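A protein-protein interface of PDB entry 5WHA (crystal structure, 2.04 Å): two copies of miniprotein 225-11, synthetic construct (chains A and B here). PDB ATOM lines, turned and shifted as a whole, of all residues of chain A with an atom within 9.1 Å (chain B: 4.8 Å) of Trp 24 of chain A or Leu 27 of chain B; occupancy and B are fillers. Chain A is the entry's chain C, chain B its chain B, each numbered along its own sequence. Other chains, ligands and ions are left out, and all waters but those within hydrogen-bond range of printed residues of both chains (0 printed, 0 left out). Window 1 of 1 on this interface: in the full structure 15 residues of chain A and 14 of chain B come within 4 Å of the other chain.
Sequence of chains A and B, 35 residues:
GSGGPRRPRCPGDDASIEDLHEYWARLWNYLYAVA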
ATOM      1  N   PRO A   8      24.322  17.207 -16.981  1.00  0.00           N
ATOM      2  CA  PRO A   8      24.433  17.753 -18.338  1.00  0.00           C
ATOM      3  C   PRO A   8      24.038  19.225 -18.405  1.00  0.00           C
ATOM      4  O   PRO A   8      23.189  19.669 -17.632  1.00  0.00           O
ATOM      5  CB  PRO A   8      23.456  16.889 -19.140  1.00  0.00           C
ATOM      6  CG  PRO A   8      22.437  16.463 -18.138  1.00  0.00           C
ATOM      7  CD  PRO A   8      23.192  16.270 -16.852  1.00  0.00           C
ATOM      8  N   ARG A   9      24.655  19.970 -19.315  1.00  0.00           N
ATOM      9  CA  ARG A   9      24.310  21.372 -19.512  1.00  0.00           C
ATOM     10  C   ARG A   9      23.329  21.532 -20.666  1.00  0.00           C
ATOM     11  O   ARG A   9      23.562  21.033 -21.767  1.00  0.00           O
ATOM     12  CB  ARG A   9      25.565  22.214 -19.763  1.00  0.00           C
ATOM     13  CG  ARG A   9      26.163  22.817 -18.501  1.00  0.00           C
ATOM     14  CD  ARG A   9      27.308  23.773 -18.809  1.00  0.00           C
ATOM     15  NE  ARG A   9      28.516  23.074 -19.243  1.00  0.00           N
ATOM     16  CZ  ARG A   9      28.950  23.032 -20.498  1.00  0.00           C
ATOM     17  NH1 ARG A   9      28.279  23.655 -21.458  1.00  0.00           N
ATOM     18  NH2 ARG A   9      30.061  22.370 -20.794  1.00  0.00           N
ATOM     19  N   CYS A  10      22.228  22.228 -20.404  1.00  0.00           N
ATOM     20  CA  CYS A  10      21.211  22.458 -21.422  1.00  0.00           C
ATOM     21  C   CYS A  10      21.726  23.396 -22.505  1.00  0.00           C
ATOM     22  O   CYS A  10      22.200  24.494 -22.208  1.00  0.00           O
ATOM     23  CB  CYS A  10      19.938  23.030 -20.795  1.00  0.00           C
ATOM     24  SG  CYS A  10      18.620  23.382 -21.985  1.00  0.00           S
ATOM     25  N   PRO A  11      21.639  22.961 -23.770  1.00  0.00           N
ATOM     26  CA  PRO A  11      22.052  23.793 -24.902  1.00  0.00           C
ATOM     27  C   PRO A  11      21.082  24.949 -25.115  1.00  0.00           C
ATOM     28  O   PRO A  11      19.893  24.809 -24.825  1.00  0.00           O
ATOM     29  CB  PRO A  11      22.026  22.817 -26.079  1.00  0.00           C
ATOM     30  CG  PRO A  11      20.997  21.812 -25.697  1.00  0.00           C
ATOM     31  CD  PRO A  11      21.116  21.654 -24.206  1.00  0.00           C
ATOM     32  N   SER A  16      19.757  22.619 -32.003  1.00  0.00           N
ATOM     33  CA  SER A  16      18.856  21.941 -32.925  1.00  0.00           C
ATOM     34  C   SER A  16      18.042  20.878 -32.195  1.00  0.00           C
ATOM     35  O   SER A  16      18.143  20.738 -30.976  1.00  0.00           O
ATOM     36  CB  SER A  16      19.643  21.310 -34.076  1.00  0.00           C
ATOM     37  OG  SER A  16      20.573  20.354 -33.595  1.00  0.00           O
ATOM     38  N   ILE A  17      17.234  20.135 -32.943  1.00  0.00           N
ATOM     39  CA  ILE A  17      16.431  19.062 -32.368  1.00  0.00           C
ATOM     40  C   ILE A  17      17.331  17.946 -31.848  1.00  0.00           C
ATOM     41  O   ILE A  17      17.092  17.392 -30.774  1.00  0.00           O
ATOM     42  CB  ILE A  17      15.437  18.485 -33.394  1.00  0.00           C
ATOM     43  CG1 ILE A  17      14.489  19.578 -33.889  1.00  0.00           C
ATOM     44  CG2 ILE A  17      14.646  17.335 -32.787  1.00  0.00           C
ATOM     45  CD1 ILE A  17      13.645  20.193 -32.795  1.00  0.00           C
ATOM     46  N   GLU A  18      18.371  17.627 -32.610  1.00  0.00           N
ATOM     47  CA  GLU A  18      19.314  16.584 -32.224  1.00  0.00           C
ATOM     48  C   GLU A  18      20.049  16.958 -30.940  1.00  0.00           C
ATOM     49  O   GLU A  18      20.273  16.110 -30.079  1.00  0.00           O
ATOM     50  CB  GLU A  18      20.318  16.319 -33.346  1.00  0.00           C
ATOM     51  CG  GLU A  18      21.247  15.146 -33.076  1.00  0.00           C
ATOM     52  CD  GLU A  18      22.299  14.976 -34.152  1.00  0.00           C
ATOM     53  OE1 GLU A  18      22.501  15.923 -34.942  1.00  0.00           O
ATOM     54  OE2 GLU A  18      22.924  13.896 -34.210  1.00  0.00           O
ATOM     55  N   ASP A  19      20.418  18.231 -30.821  1.00  0.00           N
ATOM     56  CA  ASP A  19      21.091  18.732 -29.626  1.00  0.00           C
ATOM     57  C   ASP A  19      20.215  18.572 -28.389  1.00  0.00           C
ATOM     58  O   ASP A  19      20.712  18.312 -27.294  1.00  0.00           O
ATOM     59  CB  ASP A  19      21.480  20.202 -29.800  1.00  0.00           C
ATOM     60  CG  ASP A  19      22.508  20.410 -30.892  1.00  0.00           C
ATOM     61  OD1 ASP A  19      23.261  19.460 -31.194  1.00  0.00           O
ATOM     62  OD2 ASP A  19      22.568  21.527 -31.446  1.00  0.00           O
ATOM     63  N   LEU A  20      18.908  18.734 -28.571  1.00  0.00           N
ATOM     64  CA  LEU A  20      17.958  18.561 -27.480  1.00  0.00           C
ATOM     65  C   LEU A  20      17.729  17.083 -27.191  1.00  0.00           C
ATOM     66  O   LEU A  20      17.484  16.698 -26.048  1.00  0.00           O
ATOM     67  CB  LEU A  20      16.631  19.248 -27.805  1.00  0.00           C
ATOM     68  CG  LEU A  20      16.655  20.775 -27.872  1.00  0.00           C
ATOM     69  CD1 LEU A  20      15.303  21.309 -28.306  1.00  0.00           C
ATOM     70  CD2 LEU A  20      17.061  21.364 -26.530  1.00  0.00           C
ATOM     71  N   HIS A  21      17.810  16.259 -28.233  1.00  0.00           N
ATOM     72  CA  HIS A  21      17.657  14.817 -28.082  1.00  0.00           C
ATOM     73  C   HIS A  21      18.813  14.239 -27.275  1.00  0.00           C
ATOM     74  O   HIS A  21      18.623  13.353 -26.441  1.00  0.00           O
ATOM     75  CB  HIS A  21      17.576  14.130 -29.445  1.00  0.00           C
ATOM     76  CG  HIS A  21      17.402  12.646 -29.361  1.00  0.00           C
ATOM     77  ND1 HIS A  21      16.165  12.045 -29.269  1.00  0.00           N
ATOM     78  CD2 HIS A  21      18.310  11.642 -29.344  1.00  0.00           C
ATOM     79  CE1 HIS A  21      16.317  10.734 -29.205  1.00  0.00           C
ATOM     80  NE2 HIS A  21      17.609  10.463 -29.250  1.00  0.00           N
ATOM     81  N   GLU A  22      20.012  14.750 -27.534  1.00  0.00           N
ATOM     82  CA  GLU A  22      21.196  14.355 -26.785  1.00  0.00           C
ATOM     83  C   GLU A  22      21.034  14.726 -25.316  1.00  0.00           C
ATOM     84  O   GLU A  22      21.213  13.889 -24.432  1.00  0.00           O
ATOM     85  CB  GLU A  22      22.448  15.016 -27.366  1.00  0.00           C
ATOM     86  CG  GLU A  22      22.758  14.605 -28.797  1.00  0.00           C
ATOM     87  CD  GLU A  22      23.713  15.560 -29.485  1.00  0.00           C
ATOM     88  OE1 GLU A  22      23.985  15.365 -30.687  1.00  0.00           O
ATOM     89  OE2 GLU A  22      24.189  16.508 -28.824  1.00  0.00           O
ATOM     90  N   TYR A  23      20.683  15.984 -25.067  1.00  0.00           N
ATOM     91  CA  TYR A  23      20.471  16.475 -23.711  1.00  0.00           C
ATOM     92  C   TYR A  23      19.310  15.751 -23.033  1.00  0.00           C
ATOM     93  O   TYR A  23      19.291  15.598 -21.812  1.00  0.00           O
ATOM     94  CB  TYR A  23      20.221  17.985 -23.723  1.00  0.00           C
ATOM     95  CG  TYR A  23      19.949  18.576 -22.358  1.00  0.00           C
ATOM     96  CD1 TYR A  23      20.907  18.522 -21.354  1.00  0.00           C
ATOM     97  CD2 TYR A  23      18.742  19.201 -22.079  1.00  0.00           C
ATOM     98  CE1 TYR A  23      20.666  19.064 -20.105  1.00  0.00           C
ATOM     99  CE2 TYR A  23      18.493  19.746 -20.835  1.00  0.00           C
ATOM    100  CZ  TYR A  23      19.457  19.676 -19.852  1.00  0.00           C
ATOM    101  OH  TYR A  23      19.208  20.221 -18.611  1.00  0.00           O
ATOM    102  N   TRP A  24      18.345  15.305 -23.832  1.00  0.00           N
ATOM    103  CA  TRP A  24      17.234  14.509 -23.320  1.00  0.00           C
ATOM    104  C   TRP A  24      17.725  13.147 -22.850  1.00  0.00           C
ATOM    105  O   TRP A  24      17.277  12.631 -21.824  1.00  0.00           O
ATOM    106  CB  TRP A  24      16.153  14.341 -24.391  1.00  0.00           C
ATOM    107  CG  TRP A  24      15.085  13.358 -24.023  1.00  0.00           C
ATOM    108  CD1 TRP A  24      13.977  13.596 -23.263  1.00  0.00           C
ATOM    109  CD2 TRP A  24      15.019  11.979 -24.408  1.00  0.00           C
ATOM    110  NE1 TRP A  24      13.228  12.450 -23.145  1.00  0.00           N
ATOM    111  CE2 TRP A  24      13.846  11.443 -23.840  1.00  0.00           C
ATOM    112  CE3 TRP A  24      15.840  11.145 -25.175  1.00  0.00           C
ATOM    113  CZ2 TRP A  24      13.473  10.110 -24.015  1.00  0.00           C
ATOM    114  CZ3 TRP A  24      15.468   9.823 -25.347  1.00  0.00           C
ATOM    115  CH2 TRP A  24      14.295   9.320 -24.770  1.00  0.00           C
ATOM    116  N   ALA A  25      18.650  12.568 -23.610  1.00  0.00           N
ATOM    117  CA  ALA A  25      19.220  11.271 -23.269  1.00  0.00           C
ATOM    118  C   ALA A  25      20.201  11.390 -22.107  1.00  0.00           C
ATOM    119  O   ALA A  25      20.296  10.491 -21.272  1.00  0.00           O
ATOM    120  CB  ALA A  25      19.906  10.659 -24.479  1.00  0.00           C
ATOM    121  N   ARG A  26      20.929  12.503 -22.059  1.00  0.00           N
ATOM    122  CA  ARG A  26      21.898  12.736 -20.994  1.00  0.00           C
ATOM    123  C   ARG A  26      21.205  13.035 -19.669  1.00  0.00           C
ATOM    124  O   ARG A  26      21.653  12.595 -18.611  1.00  0.00           O
ATOM    125  CB  ARG A  26      22.841  13.886 -21.358  1.00  0.00           C
ATOM    126  CG  ARG A  26      23.732  13.608 -22.554  1.00  0.00           C
ATOM    127  CD  ARG A  26      24.697  14.755 -22.800  1.00  0.00           C
ATOM    128  NE  ARG A  26      25.407  14.609 -24.068  1.00  0.00           N
ATOM    129  CZ  ARG A  26      26.514  13.891 -24.227  1.00  0.00           C
ATOM    130  NH1 ARG A  26      27.043  13.245 -23.196  1.00  0.00           N
ATOM    131  NH2 ARG A  26      27.091  13.816 -25.418  1.00  0.00           N
ATOM    132  N   LEU A  27      20.110  13.786 -19.734  1.00  0.00           N
ATOM    133  CA  LEU A  27      19.356  14.134 -18.537  1.00  0.00           C
ATOM    134  C   LEU A  27      18.671  12.899 -17.962  1.00  0.00           C
ATOM    135  O   LEU A  27      18.635  12.710 -16.746  1.00  0.00           O
ATOM    136  CB  LEU A  27      18.325  15.224 -18.843  1.00  0.00           C
ATOM    137  CG  LEU A  27      17.708  15.938 -17.640  1.00  0.00           C
ATOM    138  CD1 LEU A  27      18.793  16.577 -16.786  1.00  0.00           C
ATOM    139  CD2 LEU A  27      16.702  16.980 -18.099  1.00  0.00           C
ATOM    140  N   TRP A  28      18.132  12.060 -18.841  1.00  0.00           N
ATOM    141  CA  TRP A  28      17.509  10.810 -18.422  1.00  0.00           C
ATOM    142  C   TRP A  28      18.536   9.909 -17.749  1.00  0.00           C
ATOM    143  O   TRP A  28      18.269   9.313 -16.706  1.00  0.00           O
ATOM    144  CB  TRP A  28      16.876  10.089 -19.616  1.00  0.00           C
ATOM    145  CG  TRP A  28      16.219   8.790 -19.250  1.00  0.00           C
ATOM    146  CD1 TRP A  28      14.916   8.604 -18.888  1.00  0.00           C
ATOM    147  CD2 TRP A  28      16.834   7.496 -19.207  1.00  0.00           C
ATOM    148  NE1 TRP A  28      14.682   7.277 -18.623  1.00  0.00           N
ATOM    149  CE2 TRP A  28      15.845   6.575 -18.811  1.00  0.00           C
ATOM    150  CE3 TRP A  28      18.126   7.027 -19.464  1.00  0.00           C
ATOM    151  CZ2 TRP A  28      16.104   5.213 -18.667  1.00  0.00           C
ATOM    152  CZ3 TRP A  28      18.384   5.674 -19.321  1.00  0.00           C
ATOM    153  CH2 TRP A  28      17.376   4.784 -18.926  1.00  0.00           C
ATOM    154  N   ASN A  29      19.714   9.818 -18.359  1.00  0.00           N
ATOM    155  CA  ASN A  29      20.809   9.027 -17.814  1.00  0.00           C
ATOM    156  C   ASN A  29      21.288   9.575 -16.474  1.00  0.00           C
ATOM    157  O   ASN A  29      21.684   8.818 -15.587  1.00  0.00           O
ATOM    158  CB  ASN A  29      21.970   8.978 -18.809  1.00  0.00           C
ATOM    159  CG  ASN A  29      23.182   8.255 -18.257  1.00  0.00           C
ATOM    160  OD1 ASN A  29      24.109   8.879 -17.739  1.00  0.00           O
ATOM    161  ND2 ASN A  29      23.182   6.931 -18.365  1.00  0.00           N
ATOM    162  N   TYR A  30      21.244  10.896 -16.333  1.00  0.00           N
ATOM    163  CA  TYR A  30      21.657  11.553 -15.098  1.00  0.00           C
ATOM    164  C   TYR A  30      20.617  11.379 -13.997  1.00  0.00           C
ATOM    165  O   TYR A  30      20.952  11.024 -12.867  1.00  0.00           O
ATOM    166  CB  TYR A  30      21.915  13.041 -15.346  1.00  0.00           C
ATOM    167  CG  TYR A  30      22.193  13.836 -14.090  1.00  0.00           C
ATOM    168  CD1 TYR A  30      23.427  13.763 -13.457  1.00  0.00           C
ATOM    169  CD2 TYR A  30      21.224  14.667 -13.542  1.00  0.00           C
ATOM    170  CE1 TYR A  30      23.686  14.490 -12.309  1.00  0.00           C
ATOM    171  CE2 TYR A  30      21.474  15.397 -12.395  1.00  0.00           C
ATOM    172  CZ  TYR A  30      22.707  15.307 -11.783  1.00  0.00           C
ATOM    173  OH  TYR A  30      22.960  16.033 -10.642  1.00  0.00           O
ATOM    174  N   LEU A  31      19.355  11.630 -14.333  1.00  0.00           N
ATOM    175  CA  LEU A  31      18.266  11.522 -13.367  1.00  0.00           C
ATOM    176  C   LEU A  31      18.058  10.083 -12.899  1.00  0.00           C
ATOM    177  O   LEU A  31      17.512   9.844 -11.822  1.00  0.00           O
ATOM    178  CB  LEU A  31      16.967  12.072 -13.964  1.00  0.00           C
ATOM    179  CG  LEU A  31      16.911  13.586 -14.187  1.00  0.00           C
ATOM    180  CD1 LEU A  31      15.652  13.973 -14.945  1.00  0.00           C
ATOM    181  CD2 LEU A  31      16.994  14.332 -12.863  1.00  0.00           C
ATOM    182  N   TYR A  32      18.496   9.129 -13.715  1.00  0.00           N
ATOM    183  CA  TYR A  32      18.393   7.716 -13.368  1.00  0.00           C
ATOM    184  C   TYR A  32      19.461   7.323 -12.352  1.00  0.00           C
ATOM    185  O   TYR A  32      19.170   6.674 -11.349  1.00  0.00           O
ATOM    186  CB  TYR A  32      18.511   6.845 -14.623  1.00  0.00           C
ATOM    187  CG  TYR A  32      18.559   5.359 -14.346  1.00  0.00           C
ATOM    188  CD1 TYR A  32      17.395   4.637 -14.117  1.00  0.00           C
ATOM    189  CD2 TYR A  32      19.768   4.675 -14.320  1.00  0.00           C
ATOM    190  CE1 TYR A  32      17.434   3.278 -13.865  1.00  0.00           C
ATOM    191  CE2 TYR A  32      19.817   3.318 -14.069  1.00  0.00           C
ATOM    192  CZ  TYR A  32      18.647   2.624 -13.841  1.00  0.00           C
ATOM    193  OH  TYR A  32      18.692   1.272 -13.592  1.00  0.00           O
ATOM    194  N   PRO B   8      10.348  24.068 -24.627  1.00  0.00           N
ATOM    195  CA  PRO B   8      10.483  24.436 -23.213  1.00  0.00           C
ATOM    196  C   PRO B   8      11.847  25.055 -22.921  1.00  0.00           C
ATOM    197  O   PRO B   8      12.873  24.478 -23.282  1.00  0.00           O
ATOM    198  CB  PRO B   8      10.315  23.100 -22.485  1.00  0.00           C
ATOM    199  CG  PRO B   8      10.733  22.074 -23.484  1.00  0.00           C
ATOM    200  CD  PRO B   8      10.299  22.608 -24.818  1.00  0.00           C
ATOM    201  N   TYR B  23      11.248  19.490 -16.294  1.00  0.00           N
ATOM    202  CA  TYR B  23      11.721  19.883 -17.616  1.00  0.00           C
ATOM    203  C   TYR B  23      11.799  18.694 -18.567  1.00  0.00           C
ATOM    204  O   TYR B  23      11.402  18.793 -19.728  1.00  0.00           O
ATOM    205  CB  TYR B  23      13.092  20.559 -17.514  1.00  0.00           C
ATOM    206  CG  TYR B  23      13.724  20.865 -18.855  1.00  0.00           C
ATOM    207  CD1 TYR B  23      13.427  22.040 -19.532  1.00  0.00           C
ATOM    208  CD2 TYR B  23      14.620  19.980 -19.443  1.00  0.00           C
ATOM    209  CE1 TYR B  23      14.002  22.324 -20.756  1.00  0.00           C
ATOM    210  CE2 TYR B  23      15.195  20.255 -20.668  1.00  0.00           C
ATOM    211  CZ  TYR B  23      14.884  21.429 -21.319  1.00  0.00           C
ATOM    212  OH  TYR B  23      15.459  21.707 -22.537  1.00  0.00           O
ATOM    213  N   TRP B  24      12.318  17.575 -18.069  1.00  0.00           N
ATOM    214  CA  TRP B  24      12.506  16.382 -18.887  1.00  0.00           C
ATOM    215  C   TRP B  24      11.184  15.880 -19.456  1.00  0.00           C
ATOM    216  O   TRP B  24      11.126  15.419 -20.595  1.00  0.00           O
ATOM    217  CB  TRP B  24      13.182  15.274 -18.074  1.00  0.00           C
ATOM    218  CG  TRP B  24      13.509  14.062 -18.890  1.00  0.00           C
ATOM    219  CD1 TRP B  24      14.666  13.820 -19.570  1.00  0.00           C
ATOM    220  CD2 TRP B  24      12.663  12.927 -19.120  1.00  0.00           C
ATOM    221  NE1 TRP B  24      14.596  12.604 -20.207  1.00  0.00           N
ATOM    222  CE2 TRP B  24      13.377  12.037 -19.947  1.00  0.00           C
ATOM    223  CE3 TRP B  24      11.374  12.580 -18.706  1.00  0.00           C
ATOM    224  CZ2 TRP B  24      12.843  10.820 -20.369  1.00  0.00           C
ATOM    225  CZ3 TRP B  24      10.846  11.371 -19.126  1.00  0.00           C
ATOM    226  CH2 TRP B  24      11.581  10.505 -19.948  1.00  0.00           C
ATOM    227  N   ALA B  25      10.127  15.973 -18.656  1.00  0.00           N
ATOM    228  CA  ALA B  25       8.798  15.554 -19.086  1.00  0.00           C
ATOM    229  C   ALA B  25       8.258  16.488 -20.165  1.00  0.00           C
ATOM    230  O   ALA B  25       7.508  16.067 -21.048  1.00  0.00           O
ATOM    231  CB  ALA B  25       7.848  15.504 -17.901  1.00  0.00           C
ATOM    232  N   ARG B  26       8.648  17.755 -20.087  1.00  0.00           N
ATOM    233  CA  ARG B  26       8.253  18.748 -21.077  1.00  0.00           C
ATOM    234  C   ARG B  26       8.986  18.513 -22.392  1.00  0.00           C
ATOM    235  O   ARG B  26       8.387  18.549 -23.466  1.00  0.00           O
ATOM    236  CB  ARG B  26       8.535  20.161 -20.562  1.00  0.00           C
ATOM    237  CG  ARG B  26       7.789  20.524 -19.293  1.00  0.00           C
ATOM    238  CD  ARG B  26       6.512  21.282 -19.599  1.00  0.00           C
ATOM    239  NE  ARG B  26       6.782  22.494 -20.367  1.00  0.00           N
ATOM    240  CZ  ARG B  26       7.215  23.634 -19.839  1.00  0.00           C
ATOM    241  NH1 ARG B  26       7.433  23.722 -18.534  1.00  0.00           N
ATOM    242  NH2 ARG B  26       7.435  24.686 -20.616  1.00  0.00           N
ATOM    243  N   LEU B  27      10.290  18.273 -22.291  1.00  0.00           N
ATOM    244  CA  LEU B  27      11.125  18.023 -23.460  1.00  0.00           C
ATOM    245  C   LEU B  27      10.784  16.676 -24.093  1.00  0.00           C
ATOM    246  O   LEU B  27      11.004  16.464 -25.287  1.00  0.00           O
ATOM    247  CB  LEU B  27      12.605  18.070 -23.072  1.00  0.00           C
ATOM    248  CG  LEU B  27      13.630  18.000 -24.203  1.00  0.00           C
ATOM    249  CD1 LEU B  27      13.395  19.115 -25.207  1.00  0.00           C
ATOM    250  CD2 LEU B  27      15.044  18.064 -23.644  1.00  0.00           C
ATOM    251  N   TRP B  28      10.246  15.771 -23.282  1.00  0.00           N
ATOM    252  CA  TRP B  28       9.844  14.449 -23.749  1.00  0.00           C
ATOM    253  C   TRP B  28       8.738  14.554 -24.796  1.00  0.00           C
ATOM    254  O   TRP B  28       8.812  13.935 -25.858  1.00  0.00           O
ATOM    255  CB  TRP B  28       9.374  13.590 -22.571  1.00  0.00           C
ATOM    256  CG  TRP B  28       9.299  12.124 -22.869  1.00  0.00           C
ATOM    257  CD1 TRP B  28       9.893  11.466 -23.905  1.00  0.00           C
ATOM    258  CD2 TRP B  28       8.586  11.134 -22.118  1.00  0.00           C
ATOM    259  NE1 TRP B  28       9.595  10.125 -23.844  1.00  0.00           N
ATOM    260  CE2 TRP B  28       8.793   9.896 -22.756  1.00  0.00           C
ATOM    261  CE3 TRP B  28       7.793  11.175 -20.966  1.00  0.00           C
ATOM    262  CZ2 TRP B  28       8.237   8.709 -22.284  1.00  0.00           C
ATOM    263  CZ3 TRP B  28       7.241   9.994 -20.498  1.00  0.00           C
ATOM    264  CH2 TRP B  28       7.466   8.779 -21.156  1.00  0.00           C
ATOM    265  N   ASN B  29       7.718  15.349 -24.487  1.00  0.00           N
ATOM    266  CA  ASN B  29       6.582  15.532 -25.382  1.00  0.00           C
ATOM    267  C   ASN B  29       6.909  16.426 -26.573  1.00  0.00           C
ATOM    268  O   ASN B  29       6.374  16.235 -27.664  1.00  0.00           O
ATOM    269  CB  ASN B  29       5.392  16.113 -24.615  1.00  0.00           C
ATOM    270  CG  ASN B  29       4.820  15.142 -23.602  1.00  0.00           C
ATOM    271  OD1 ASN B  29       3.860  14.424 -23.885  1.00  0.00           O
ATOM    272  ND2 ASN B  29       5.409  15.115 -22.412  1.00  0.00           N
ATOM    273  N   TYR B  30       7.783  17.404 -26.357  1.00  0.00           N
ATOM    274  CA  TYR B  30       8.148  18.345 -27.411  1.00  0.00           C
ATOM    275  C   TYR B  30       8.938  17.662 -28.523  1.00  0.00           C
ATOM    276  O   TYR B  30       8.625  17.820 -29.704  1.00  0.00           O
ATOM    277  CB  TYR B  30       8.958  19.512 -26.838  1.00  0.00           C
ATOM    278  CG  TYR B  30       9.525  20.431 -27.897  1.00  0.00           C
ATOM    279  CD1 TYR B  30       8.708  21.324 -28.579  1.00  0.00           C
ATOM    280  CD2 TYR B  30      10.876  20.405 -28.216  1.00  0.00           C
ATOM    281  CE1 TYR B  30       9.221  22.163 -29.550  1.00  0.00           C
ATOM    282  CE2 TYR B  30      11.398  21.240 -29.186  1.00  0.00           C
ATOM    283  CZ  TYR B  30      10.566  22.117 -29.850  1.00  0.00           C
ATOM    284  OH  TYR B  30      11.080  22.952 -30.815  1.00  0.00           O
ATOM    285  N   LEU B  31       9.959  16.906 -28.138  1.00  0.00           N
ATOM    286  CA  LEU B  31      10.811  16.217 -29.099  1.00  0.00           C
ATOM    287  C   LEU B  31      10.031  15.191 -29.917  1.00  0.00           C
ATOM    288  O   LEU B  31      10.342  14.951 -31.084  1.00  0.00           O
ATOM    289  CB  LEU B  31      11.979  15.539 -28.381  1.00  0.00           C
ATOM    290  CG  LEU B  31      13.068  16.464 -27.834  1.00  0.00           C
ATOM    291  CD1 LEU B  31      14.144  15.665 -27.121  1.00  0.00           C
ATOM    292  CD2 LEU B  31      13.671  17.302 -28.952  1.00  0.00           C
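Hydrophobic or aromatic side chains of chain B within 4 Å of the printed part of chain A: Tyr 23, Trp 24, Leu 27, Trp 28 and Leu 31. Of the 21 printed residues of chain A, 8 touch a printed residue of chain B. Hydrophobic or aromatic side chains of chain A within 4 Å of the printed part of chain B: Ile 17, Leu 20, Tyr 23, Trp 24, Leu 27 and Trp 28. Among the printed residues, no Asp or Glu carboxylate lies within 4 Å of a Lys or Arg side-chain nitrogen of the other chain.
Trp 24 of chain B touches its own counterpart, Trp 24 of chain A. Trp 24 of chain A touches Trp 28 of chain B, and with the chains exchanged Trp 28 of chain A touches Trp 24 of chain B. Trp 24 of chain A touches Leu 31 of chain B, but with the chains exchanged Leu 31 of chain A does not touch Trp 24 of chain B (4.2 Å). Leu 27 of chain A touches Tyr 23 of chain B, but with the chains exchanged Tyr 23 of chain A does not touch Leu 27 of chain B (4.2 Å). Positions printed for both chains: 8, 23, 24, 25, 26, 27, 28, 29, 30 and 31.
The side-chain hydroxyl (OH) of Tyr 23 of chain B lies within hydrogen-bond range of the side-chain sulfur (SG) of Cys 10 of chain A, 3.6 Å away. NE1 of Trp 24 of chain B is in hydrogen-bond range of O of Trp 24 of chain A, at 3.1 Å.
Of the printed residues of chain B, Trp 24 of chain A touches Trp 24 (3.1 Å), Leu 27 (3.96 Å), Trp 28 (3.6 Å) and Leu 31 (3.6 Å). Leu 27 of chain B touches two residues of chain A. Of the printed residues of chain A, Tyr 23 of chain B touches Cys 10, Tyr 23 and Leu 27. Printed residues of chain B within 4 Å of Ile 17 of chain A: Leu 31. The nearest residue of chain A that does not touch Leu 27 of chain B is Tyr 23 of chain A (4.2 Å). The nearest printed residue of chain B that does not touch Trp 28 of chain A is Trp 28 of chain B (7.4 Å).
Among the printed residues, merely in contact across the chains: Ile 17 of chain A with Leu 31 of chain B, Leu 20 of chain A with Leu 27 of chain B, Leu 20 of chain A with Leu 31 of chain B, His 21 of chain A with Leu 31 of chain B, Tyr 23 of chain A with Tyr 23 of chain B, Trp 24 of chain A with Leu 27 of chain B, Trp 24 of chain A with Trp 28 of chain B, Trp 24 of chain A with Leu 31 of chain B, Leu 27 of chain A with Tyr 23 of chain B, Leu 27 of chain A with Trp 24 of chain B and Trp 28 of chain A with Trp 24 of chain B.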
